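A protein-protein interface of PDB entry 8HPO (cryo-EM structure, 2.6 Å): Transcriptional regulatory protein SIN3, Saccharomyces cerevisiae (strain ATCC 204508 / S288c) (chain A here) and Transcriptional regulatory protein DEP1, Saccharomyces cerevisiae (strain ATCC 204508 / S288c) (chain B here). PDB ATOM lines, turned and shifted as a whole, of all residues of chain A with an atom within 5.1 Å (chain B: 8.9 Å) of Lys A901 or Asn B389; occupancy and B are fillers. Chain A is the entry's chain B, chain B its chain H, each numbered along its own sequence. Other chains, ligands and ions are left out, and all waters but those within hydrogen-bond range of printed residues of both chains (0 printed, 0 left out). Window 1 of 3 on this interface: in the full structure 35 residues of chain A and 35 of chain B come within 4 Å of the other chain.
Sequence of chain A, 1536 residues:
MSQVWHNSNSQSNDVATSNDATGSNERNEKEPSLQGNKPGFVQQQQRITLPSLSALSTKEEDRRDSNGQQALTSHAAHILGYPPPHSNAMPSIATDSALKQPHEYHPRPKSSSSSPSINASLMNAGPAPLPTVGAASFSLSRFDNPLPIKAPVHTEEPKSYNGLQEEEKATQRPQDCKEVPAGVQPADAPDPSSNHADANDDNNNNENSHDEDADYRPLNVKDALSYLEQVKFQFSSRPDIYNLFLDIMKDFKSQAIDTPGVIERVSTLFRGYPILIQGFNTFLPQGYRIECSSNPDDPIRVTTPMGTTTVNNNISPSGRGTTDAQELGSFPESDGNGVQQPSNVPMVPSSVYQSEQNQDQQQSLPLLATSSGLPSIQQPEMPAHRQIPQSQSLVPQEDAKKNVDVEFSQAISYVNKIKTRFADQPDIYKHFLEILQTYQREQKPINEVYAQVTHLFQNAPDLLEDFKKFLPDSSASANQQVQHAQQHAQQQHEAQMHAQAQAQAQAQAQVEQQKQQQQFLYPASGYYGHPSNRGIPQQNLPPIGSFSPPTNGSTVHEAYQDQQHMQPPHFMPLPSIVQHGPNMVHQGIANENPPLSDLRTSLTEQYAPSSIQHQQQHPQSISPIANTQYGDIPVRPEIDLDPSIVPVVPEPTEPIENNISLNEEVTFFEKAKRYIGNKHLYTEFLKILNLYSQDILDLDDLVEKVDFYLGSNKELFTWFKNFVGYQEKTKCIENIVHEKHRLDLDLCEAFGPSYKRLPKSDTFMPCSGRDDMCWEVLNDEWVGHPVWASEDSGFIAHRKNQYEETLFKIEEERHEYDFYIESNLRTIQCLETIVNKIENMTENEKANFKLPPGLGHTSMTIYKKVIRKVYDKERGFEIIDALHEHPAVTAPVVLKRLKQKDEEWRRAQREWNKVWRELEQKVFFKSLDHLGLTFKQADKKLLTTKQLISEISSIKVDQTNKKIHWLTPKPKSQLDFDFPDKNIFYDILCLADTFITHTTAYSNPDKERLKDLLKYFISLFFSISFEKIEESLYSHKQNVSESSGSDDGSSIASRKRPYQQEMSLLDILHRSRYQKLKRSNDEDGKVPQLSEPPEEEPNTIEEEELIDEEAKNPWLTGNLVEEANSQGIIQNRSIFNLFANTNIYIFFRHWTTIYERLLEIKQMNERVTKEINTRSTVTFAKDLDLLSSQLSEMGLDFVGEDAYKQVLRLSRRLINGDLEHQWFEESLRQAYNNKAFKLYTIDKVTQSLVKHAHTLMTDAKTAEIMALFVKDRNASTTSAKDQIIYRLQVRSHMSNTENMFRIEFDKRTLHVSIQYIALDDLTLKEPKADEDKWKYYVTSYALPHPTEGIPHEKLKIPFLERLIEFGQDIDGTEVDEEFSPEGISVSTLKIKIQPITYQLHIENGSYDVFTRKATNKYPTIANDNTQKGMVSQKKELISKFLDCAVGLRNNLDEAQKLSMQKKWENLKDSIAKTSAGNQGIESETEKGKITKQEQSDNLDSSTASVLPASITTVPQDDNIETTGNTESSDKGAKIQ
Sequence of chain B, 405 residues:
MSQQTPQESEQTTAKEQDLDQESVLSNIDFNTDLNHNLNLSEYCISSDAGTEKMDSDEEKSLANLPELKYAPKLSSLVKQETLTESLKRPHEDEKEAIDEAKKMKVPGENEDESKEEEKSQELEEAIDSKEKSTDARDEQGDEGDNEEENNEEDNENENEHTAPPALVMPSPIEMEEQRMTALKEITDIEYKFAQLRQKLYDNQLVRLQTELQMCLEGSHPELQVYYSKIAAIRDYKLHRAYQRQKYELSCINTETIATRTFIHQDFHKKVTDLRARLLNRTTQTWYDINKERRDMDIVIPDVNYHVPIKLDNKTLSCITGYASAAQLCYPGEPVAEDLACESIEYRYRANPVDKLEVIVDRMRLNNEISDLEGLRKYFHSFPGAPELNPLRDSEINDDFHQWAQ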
ATOM      1  N   ASN A 824      -0.060  -7.807 -22.880  1.00  0.00           N
ATOM      2  CA  ASN A 824      -0.911  -7.494 -21.740  1.00  0.00           C
ATOM      3  C   ASN A 824      -1.823  -8.667 -21.408  1.00  0.00           C
ATOM      4  O   ASN A 824      -2.039  -8.986 -20.234  1.00  0.00           O
ATOM      5  CB  ASN A 824      -1.719  -6.230 -22.023  1.00  0.00           C
ATOM      6  CG  ASN A 824      -2.693  -5.898 -20.917  1.00  0.00           C
ATOM      7  OD1 ASN A 824      -3.897  -5.852 -21.132  1.00  0.00           O
ATOM      8  ND2 ASN A 824      -2.174  -5.646 -19.732  1.00  0.00           N
ATOM      9  N   VAL A 870       2.047   0.348 -18.062  1.00  0.00           N
ATOM     10  CA  VAL A 870       0.709   0.633 -17.573  1.00  0.00           C
ATOM     11  C   VAL A 870       0.743   1.768 -16.568  1.00  0.00           C
ATOM     12  O   VAL A 870      -0.172   2.597 -16.535  1.00  0.00           O
ATOM     13  CB  VAL A 870       0.059  -0.625 -16.977  1.00  0.00           C
ATOM     14  CG1 VAL A 870      -1.302  -0.291 -16.378  1.00  0.00           C
ATOM     15  CG2 VAL A 870      -0.076  -1.692 -18.033  1.00  0.00           C
ATOM     16  N   ARG A 897      -6.293  -3.513 -12.957  1.00  0.00           N
ATOM     17  CA  ARG A 897      -5.949  -2.414 -13.849  1.00  0.00           C
ATOM     18  C   ARG A 897      -5.453  -2.881 -15.211  1.00  0.00           C
ATOM     19  O   ARG A 897      -5.759  -2.244 -16.221  1.00  0.00           O
ATOM     20  CB  ARG A 897      -4.902  -1.526 -13.180  1.00  0.00           C
ATOM     21  CG  ARG A 897      -5.405  -0.946 -11.879  1.00  0.00           C
ATOM     22  CD  ARG A 897      -5.081   0.510 -11.761  1.00  0.00           C
ATOM     23  NE  ARG A 897      -6.044   1.219 -10.932  1.00  0.00           N
ATOM     24  CZ  ARG A 897      -7.221   1.643 -11.370  1.00  0.00           C
ATOM     25  NH1 ARG A 897      -7.575   1.423 -12.626  1.00  0.00           N
ATOM     26  NH2 ARG A 897      -8.044   2.283 -10.556  1.00  0.00           N
ATOM     27  N   LEU A 898      -4.698  -3.980 -15.266  1.00  0.00           N
ATOM     28  CA  LEU A 898      -4.431  -4.634 -16.543  1.00  0.00           C
ATOM     29  C   LEU A 898      -5.730  -4.989 -17.257  1.00  0.00           C
ATOM     30  O   LEU A 898      -5.804  -4.961 -18.492  1.00  0.00           O
ATOM     31  CB  LEU A 898      -3.593  -5.894 -16.324  1.00  0.00           C
ATOM     32  CG  LEU A 898      -2.210  -5.763 -15.686  1.00  0.00           C
ATOM     33  CD1 LEU A 898      -1.450  -7.063 -15.797  1.00  0.00           C
ATOM     34  CD2 LEU A 898      -1.434  -4.649 -16.334  1.00  0.00           C
ATOM     35  N   LYS A 899      -6.776  -5.297 -16.491  1.00  0.00           N
ATOM     36  CA  LYS A 899      -8.051  -5.660 -17.092  1.00  0.00           C
ATOM     37  C   LYS A 899      -8.836  -4.431 -17.529  1.00  0.00           C
ATOM     38  O   LYS A 899      -9.881  -4.564 -18.172  1.00  0.00           O
ATOM     39  CB  LYS A 899      -8.870  -6.498 -16.111  1.00  0.00           C
ATOM     40  CG  LYS A 899      -8.342  -7.908 -15.928  1.00  0.00           C
ATOM     41  CD  LYS A 899      -9.314  -8.765 -15.152  1.00  0.00           C
ATOM     42  CE  LYS A 899      -9.009 -10.235 -15.338  1.00  0.00           C
ATOM     43  NZ  LYS A 899     -10.126 -11.089 -14.862  1.00  0.00           N
ATOM     44  N   GLN A 900      -8.370  -3.238 -17.171  1.00  0.00           N
ATOM     45  CA  GLN A 900      -8.894  -2.029 -17.790  1.00  0.00           C
ATOM     46  C   GLN A 900      -8.101  -1.694 -19.037  1.00  0.00           C
ATOM     47  O   GLN A 900      -8.666  -1.298 -20.065  1.00  0.00           O
ATOM     48  CB  GLN A 900      -8.833  -0.866 -16.809  1.00  0.00           C
ATOM     49  CG  GLN A 900     -10.096  -0.646 -16.031  1.00  0.00           C
ATOM     50  CD  GLN A 900      -9.937   0.440 -14.995  1.00  0.00           C
ATOM     51  OE1 GLN A 900     -10.501   0.360 -13.904  1.00  0.00           O
ATOM     52  NE2 GLN A 900      -9.160   1.463 -15.326  1.00  0.00           N
ATOM     53  N   LYS A 901      -6.783  -1.849 -18.958  1.00  0.00           N
ATOM     54  CA  LYS A 901      -5.926  -1.444 -20.058  1.00  0.00           C
ATOM     55  C   LYS A 901      -6.095  -2.349 -21.263  1.00  0.00           C
ATOM     56  O   LYS A 901      -5.956  -1.885 -22.392  1.00  0.00           O
ATOM     57  CB  LYS A 901      -4.473  -1.412 -19.598  1.00  0.00           C
ATOM     58  CG  LYS A 901      -4.000  -0.036 -19.173  1.00  0.00           C
ATOM     59  CD  LYS A 901      -5.165   0.908 -18.956  1.00  0.00           C
ATOM     60  CE  LYS A 901      -4.707   2.334 -18.800  1.00  0.00           C
ATOM     61  NZ  LYS A 901      -5.848   3.286 -18.824  1.00  0.00           N
ATOM     62  N   ASP A 902      -6.439  -3.619 -21.059  1.00  0.00           N
ATOM     63  CA  ASP A 902      -6.716  -4.490 -22.196  1.00  0.00           C
ATOM     64  C   ASP A 902      -7.921  -3.993 -22.984  1.00  0.00           C
ATOM     65  O   ASP A 902      -7.856  -3.806 -24.209  1.00  0.00           O
ATOM     66  CB  ASP A 902      -6.950  -5.918 -21.714  1.00  0.00           C
ATOM     67  CG  ASP A 902      -7.179  -6.879 -22.849  1.00  0.00           C
ATOM     68  OD1 ASP A 902      -8.333  -7.304 -23.046  1.00  0.00           O
ATOM     69  OD2 ASP A 902      -6.205  -7.199 -23.553  1.00  0.00           O
ATOM     70  N   GLU A 903      -9.029  -3.765 -22.281  1.00  0.00           N
ATOM     71  CA  GLU A 903     -10.250  -3.273 -22.904  1.00  0.00           C
ATOM     72  C   GLU A 903     -10.004  -1.956 -23.631  1.00  0.00           C
ATOM     73  O   GLU A 903     -10.362  -1.797 -24.809  1.00  0.00           O
ATOM     74  CB  GLU A 903     -11.318  -3.114 -21.824  1.00  0.00           C
ATOM     75  CG  GLU A 903     -12.721  -2.864 -22.313  1.00  0.00           C
ATOM     76  CD  GLU A 903     -13.339  -4.077 -22.971  1.00  0.00           C
ATOM     77  OE1 GLU A 903     -14.384  -3.921 -23.638  1.00  0.00           O
ATOM     78  OE2 GLU A 903     -12.780  -5.185 -22.824  1.00  0.00           O
ATOM     79  N   GLU A 904      -9.338  -1.016 -22.951  1.00  0.00           N
ATOM     80  CA  GLU A 904      -9.116   0.299 -23.540  1.00  0.00           C
ATOM     81  C   GLU A 904      -8.167   0.236 -24.727  1.00  0.00           C
ATOM     82  O   GLU A 904      -8.390   0.912 -25.736  1.00  0.00           O
ATOM     83  CB  GLU A 904      -8.596   1.262 -22.480  1.00  0.00           C
ATOM     84  CG  GLU A 904      -9.667   1.664 -21.502  1.00  0.00           C
ATOM     85  CD  GLU A 904      -9.284   2.842 -20.641  1.00  0.00           C
ATOM     86  OE1 GLU A 904      -9.429   2.746 -19.407  1.00  0.00           O
ATOM     87  OE2 GLU A 904      -8.848   3.871 -21.194  1.00  0.00           O
ATOM     88  N   TRP A 905      -7.120  -0.581 -24.653  1.00  0.00           N
ATOM     89  CA  TRP A 905      -6.146  -0.598 -25.731  1.00  0.00           C
ATOM     90  C   TRP A 905      -6.687  -1.300 -26.962  1.00  0.00           C
ATOM     91  O   TRP A 905      -6.323  -0.943 -28.090  1.00  0.00           O
ATOM     92  CB  TRP A 905      -4.865  -1.273 -25.262  1.00  0.00           C
ATOM     93  CG  TRP A 905      -4.101  -0.482 -24.273  1.00  0.00           C
ATOM     94  CD1 TRP A 905      -4.405   0.757 -23.800  1.00  0.00           C
ATOM     95  CD2 TRP A 905      -2.892  -0.874 -23.631  1.00  0.00           C
ATOM     96  NE1 TRP A 905      -3.459   1.161 -22.901  1.00  0.00           N
ATOM     97  CE2 TRP A 905      -2.518   0.174 -22.777  1.00  0.00           C
ATOM     98  CE3 TRP A 905      -2.092  -2.017 -23.687  1.00  0.00           C
ATOM     99  CZ2 TRP A 905      -1.378   0.117 -21.993  1.00  0.00           C
ATOM    100  CZ3 TRP A 905      -0.967  -2.071 -22.908  1.00  0.00           C
ATOM    101  CH2 TRP A 905      -0.614  -1.012 -22.076  1.00  0.00           C
ATOM    102  N   ARG A 906      -7.599  -2.256 -26.782  1.00  0.00           N
ATOM    103  CA  ARG A 906      -8.228  -2.861 -27.950  1.00  0.00           C
ATOM    104  C   ARG A 906      -9.223  -1.905 -28.597  1.00  0.00           C
ATOM    105  O   ARG A 906      -9.292  -1.817 -29.832  1.00  0.00           O
ATOM    106  CB  ARG A 906      -8.891  -4.177 -27.570  1.00  0.00           C
ATOM    107  CG  ARG A 906      -7.913  -5.330 -27.453  1.00  0.00           C
ATOM    108  CD  ARG A 906      -8.635  -6.626 -27.146  1.00  0.00           C
ATOM    109  NE  ARG A 906     -10.028  -6.381 -26.794  1.00  0.00           N
ATOM    110  CZ  ARG A 906     -10.575  -6.725 -25.638  1.00  0.00           C
ATOM    111  NH1 ARG A 906     -11.849  -6.459 -25.402  1.00  0.00           N
ATOM    112  NH2 ARG A 906      -9.848  -7.337 -24.720  1.00  0.00           N
ATOM    113  N   VAL B 303     -14.215  -5.924 -16.805  1.00  0.00           N
ATOM    114  CA  VAL B 303     -14.919  -4.680 -17.075  1.00  0.00           C
ATOM    115  C   VAL B 303     -15.179  -4.615 -18.566  1.00  0.00           C
ATOM    116  O   VAL B 303     -14.449  -5.202 -19.372  1.00  0.00           O
ATOM    117  CB  VAL B 303     -14.125  -3.449 -16.596  1.00  0.00           C
ATOM    118  CG1 VAL B 303     -14.041  -3.427 -15.089  1.00  0.00           C
ATOM    119  CG2 VAL B 303     -12.744  -3.462 -17.199  1.00  0.00           C
ATOM    120  N   TYR B 305     -17.161  -1.817 -21.731  1.00  0.00           N
ATOM    121  CA  TYR B 305     -17.830  -0.572 -22.045  1.00  0.00           C
ATOM    122  C   TYR B 305     -19.336  -0.779 -22.051  1.00  0.00           C
ATOM    123  O   TYR B 305     -19.827  -1.900 -22.173  1.00  0.00           O
ATOM    124  CB  TYR B 305     -17.370  -0.053 -23.404  1.00  0.00           C
ATOM    125  CG  TYR B 305     -16.036   0.649 -23.378  1.00  0.00           C
ATOM    126  CD1 TYR B 305     -15.901   1.895 -22.796  1.00  0.00           C
ATOM    127  CD2 TYR B 305     -14.914   0.067 -23.937  1.00  0.00           C
ATOM    128  CE1 TYR B 305     -14.696   2.540 -22.777  1.00  0.00           C
ATOM    129  CE2 TYR B 305     -13.700   0.707 -23.919  1.00  0.00           C
ATOM    130  CZ  TYR B 305     -13.598   1.944 -23.337  1.00  0.00           C
ATOM    131  OH  TYR B 305     -12.390   2.592 -23.316  1.00  0.00           O
ATOM    132  N   GLU B 368      -9.112  15.631 -28.298  1.00  0.00           N
ATOM    133  CA  GLU B 368      -8.148  14.822 -29.043  1.00  0.00           C
ATOM    134  C   GLU B 368      -8.165  15.162 -30.532  1.00  0.00           C
ATOM    135  O   GLU B 368      -7.109  15.247 -31.178  1.00  0.00           O
ATOM    136  CB  GLU B 368      -8.432  13.342 -28.831  1.00  0.00           C
ATOM    137  CG  GLU B 368      -7.253  12.588 -28.281  1.00  0.00           C
ATOM    138  CD  GLU B 368      -6.279  12.187 -29.355  1.00  0.00           C
ATOM    139  OE1 GLU B 368      -5.131  11.831 -29.017  1.00  0.00           O
ATOM    140  OE2 GLU B 368      -6.662  12.228 -30.540  1.00  0.00           O
ATOM    141  N   PRO B 386      -1.990   7.515 -32.292  1.00  0.00           N
ATOM    142  CA  PRO B 386      -1.745   8.011 -30.936  1.00  0.00           C
ATOM    143  C   PRO B 386      -1.305   6.916 -29.974  1.00  0.00           C
ATOM    144  O   PRO B 386      -1.637   5.741 -30.134  1.00  0.00           O
ATOM    145  CB  PRO B 386      -3.104   8.587 -30.523  1.00  0.00           C
ATOM    146  CG  PRO B 386      -3.822   8.804 -31.781  1.00  0.00           C
ATOM    147  CD  PRO B 386      -3.385   7.718 -32.692  1.00  0.00           C
ATOM    148  N   GLU B 387      -0.559   7.330 -28.961  1.00  0.00           N
ATOM    149  CA  GLU B 387       0.042   6.408 -28.022  1.00  0.00           C
ATOM    150  C   GLU B 387      -1.012   5.857 -27.069  1.00  0.00           C
ATOM    151  O   GLU B 387      -1.962   6.543 -26.686  1.00  0.00           O
ATOM    152  CB  GLU B 387       1.154   7.107 -27.240  1.00  0.00           C
ATOM    153  CG  GLU B 387       2.185   7.825 -28.111  1.00  0.00           C
ATOM    154  CD  GLU B 387       1.693   9.155 -28.674  1.00  0.00           C
ATOM    155  OE1 GLU B 387       1.634   9.304 -29.913  1.00  0.00           O
ATOM    156  OE2 GLU B 387       1.363  10.053 -27.876  1.00  0.00           O
ATOM    157  N   LEU B 388      -0.834   4.594 -26.687  1.00  0.00           N
ATOM    158  CA  LEU B 388      -1.747   3.939 -25.759  1.00  0.00           C
ATOM    159  C   LEU B 388      -1.531   4.504 -24.358  1.00  0.00           C
ATOM    160  O   LEU B 388      -0.420   4.454 -23.824  1.00  0.00           O
ATOM    161  CB  LEU B 388      -1.533   2.425 -25.781  1.00  0.00           C
ATOM    162  CG  LEU B 388      -1.649   1.692 -27.126  1.00  0.00           C
ATOM    163  CD1 LEU B 388      -1.073   0.293 -27.037  1.00  0.00           C
ATOM    164  CD2 LEU B 388      -3.077   1.643 -27.631  1.00  0.00           C
ATOM    165  N   ASN B 389      -2.590   5.034 -23.769  1.00  0.00           N
ATOM    166  CA  ASN B 389      -2.459   5.895 -22.596  1.00  0.00           C
ATOM    167  C   ASN B 389      -2.303   5.104 -21.302  1.00  0.00           C
ATOM    168  O   ASN B 389      -3.060   4.153 -21.073  1.00  0.00           O
ATOM    169  CB  ASN B 389      -3.674   6.805 -22.494  1.00  0.00           C
ATOM    170  CG  ASN B 389      -3.594   7.989 -23.423  1.00  0.00           C
ATOM    171  OD1 ASN B 389      -2.521   8.545 -23.645  1.00  0.00           O
ATOM    172  ND2 ASN B 389      -4.736   8.386 -23.976  1.00  0.00           N
ATOM    173  N   PRO B 390      -1.357   5.459 -20.438  1.00  0.00           N
ATOM    174  CA  PRO B 390      -1.288   4.890 -19.089  1.00  0.00           C
ATOM    175  C   PRO B 390      -2.292   5.569 -18.159  1.00  0.00           C
ATOM    176  O   PRO B 390      -3.145   6.344 -18.582  1.00  0.00           O
ATOM    177  CB  PRO B 390       0.154   5.181 -18.664  1.00  0.00           C
ATOM    178  CG  PRO B 390       0.871   5.565 -19.920  1.00  0.00           C
ATOM    179  CD  PRO B 390      -0.157   6.250 -20.740  1.00  0.00           C
ATOM    180  N   LEU B 391      -2.189   5.243 -16.871  1.00  0.00           N
ATOM    181  CA  LEU B 391      -3.084   5.792 -15.862  1.00  0.00           C
ATOM    182  C   LEU B 391      -2.702   7.232 -15.511  1.00  0.00           C
ATOM    183  O   LEU B 391      -1.647   7.737 -15.901  1.00  0.00           O
ATOM    184  CB  LEU B 391      -3.045   4.933 -14.606  1.00  0.00           C
ATOM    185  CG  LEU B 391      -3.643   3.537 -14.695  1.00  0.00           C
ATOM    186  CD1 LEU B 391      -3.166   2.757 -13.513  1.00  0.00           C
ATOM    187  CD2 LEU B 391      -5.150   3.612 -14.719  1.00  0.00           C
ATOM    188  N   ARG B 392      -3.574   7.901 -14.751  1.00  0.00           N
ATOM    189  CA  ARG B 392      -3.385   9.309 -14.414  1.00  0.00           C
ATOM    190  C   ARG B 392      -3.178   9.562 -12.924  1.00  0.00           C
ATOM    191  O   ARG B 392      -2.122  10.058 -12.519  1.00  0.00           O
ATOM    192  CB  ARG B 392      -4.605  10.089 -14.905  1.00  0.00           C
ATOM    193  CG  ARG B 392      -5.388   9.365 -15.977  1.00  0.00           C
ATOM    194  CD  ARG B 392      -6.558  10.197 -16.442  1.00  0.00           C
ATOM    195  NE  ARG B 392      -7.570  10.315 -15.401  1.00  0.00           N
ATOM    196  CZ  ARG B 392      -8.695   9.610 -15.377  1.00  0.00           C
ATOM    197  NH1 ARG B 392      -8.954   8.738 -16.342  1.00  0.00           N
ATOM    198  NH2 ARG B 392      -9.564   9.777 -14.390  1.00  0.00           N
ATOM    199  N   SER B 394      -5.052   7.088 -10.699  1.00  0.00           N
ATOM    200  CA  SER B 394      -5.246   5.741 -10.198  1.00  0.00           C
ATOM    201  C   SER B 394      -3.965   5.159  -9.625  1.00  0.00           C
ATOM    202  O   SER B 394      -4.034   4.272  -8.775  1.00  0.00           O
ATOM    203  CB  SER B 394      -5.787   4.856 -11.315  1.00  0.00           C
ATOM    204  OG  SER B 394      -6.657   5.592 -12.155  1.00  0.00           O
ATOM    205  N   GLU B 395      -2.799   5.649 -10.050  1.00  0.00           N
ATOM    206  CA  GLU B 395      -1.559   5.221  -9.414  1.00  0.00           C
ATOM    207  C   GLU B 395      -1.474   5.732  -7.983  1.00  0.00           C
ATOM    208  O   GLU B 395      -1.058   4.997  -7.076  1.00  0.00           O
ATOM    209  CB  GLU B 395      -0.370   5.708 -10.228  1.00  0.00           C
ATOM    210  CG  GLU B 395      -0.750   6.021 -11.646  1.00  0.00           C
ATOM    211  CD  GLU B 395       0.367   5.772 -12.614  1.00  0.00           C
ATOM    212  OE1 GLU B 395       1.533   6.047 -12.272  1.00  0.00           O
ATOM    213  OE2 GLU B 395       0.076   5.298 -13.724  1.00  0.00           O
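Asn A824 touches none of the printed residues of chain B. Printed residues of chain B within 4 Å of Val A870: Pro B390 (3.4 Å), Leu B391 (3.3 Å) and Glu B395 (3.9 Å). Lys A901 touches one residue of chain B. Of the printed residues of chain B, Trp A905 touches Leu B388 and Asn B389. Asn B389 touches two residues of chain A. The nearest residue of chain B that does not touch Lys A901 is Pro B390 (4.1 Å). The nearest printed residue of chain A that does not touch Val B303 is Gln A900 (4.04 Å).
Val A870 touches Pro B390 (O to CB, 3.4 Å). OE2 of Glu B395 touches O of Val A870 (3.9 Å). CD of Arg A897 touches CD1 of Leu B391 (3.4 Å). Arg A897 touches Ser B394 (NH2 to CB, 3.5 Å). O of Lys A899 touches CG2 of Val B303, 3.2 Å away. Lys A901 touches Asn B389 (CE to O, 3.3 Å). Glu A903 touches Val B303. OE1 of Glu A903 touches N of Tyr B305, 3.97 Å away. Tyr B305 touches Glu A904 (OH to CG, 3.4 Å). Asn B389 touches Trp A905.
O of Val A870 lies within hydrogen-bond range of N of Leu B391, 3.3 Å away.
NE2 of Gln A900 lies close to NH1 of Arg A897. The side-chain amino group (NZ) of Lys A901 is in salt-bridge range of the side-chain carboxylate (OE1) of Glu A904. The side-chain carboxylate of Glu A903 is in salt-bridge range of the guanidinium group of Arg A906 (3.0 Å).
Of the 12 printed residues of chain B, 8 touch a printed residue of chain A. Printed residues of chain B that touch a printed residue of chain A: Val B303, Tyr B305, Leu B388, Asn B389, Pro B390, Leu B391, Ser B394 and Glu B395. Hydrophobic or aromatic side chains of chain B that line the printed part of chain A: Val B303, Tyr B305, Leu B388, Pro B390 and Leu B391. Of the 12 printed residues of chain A, 7 touch a printed residue of chain B.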
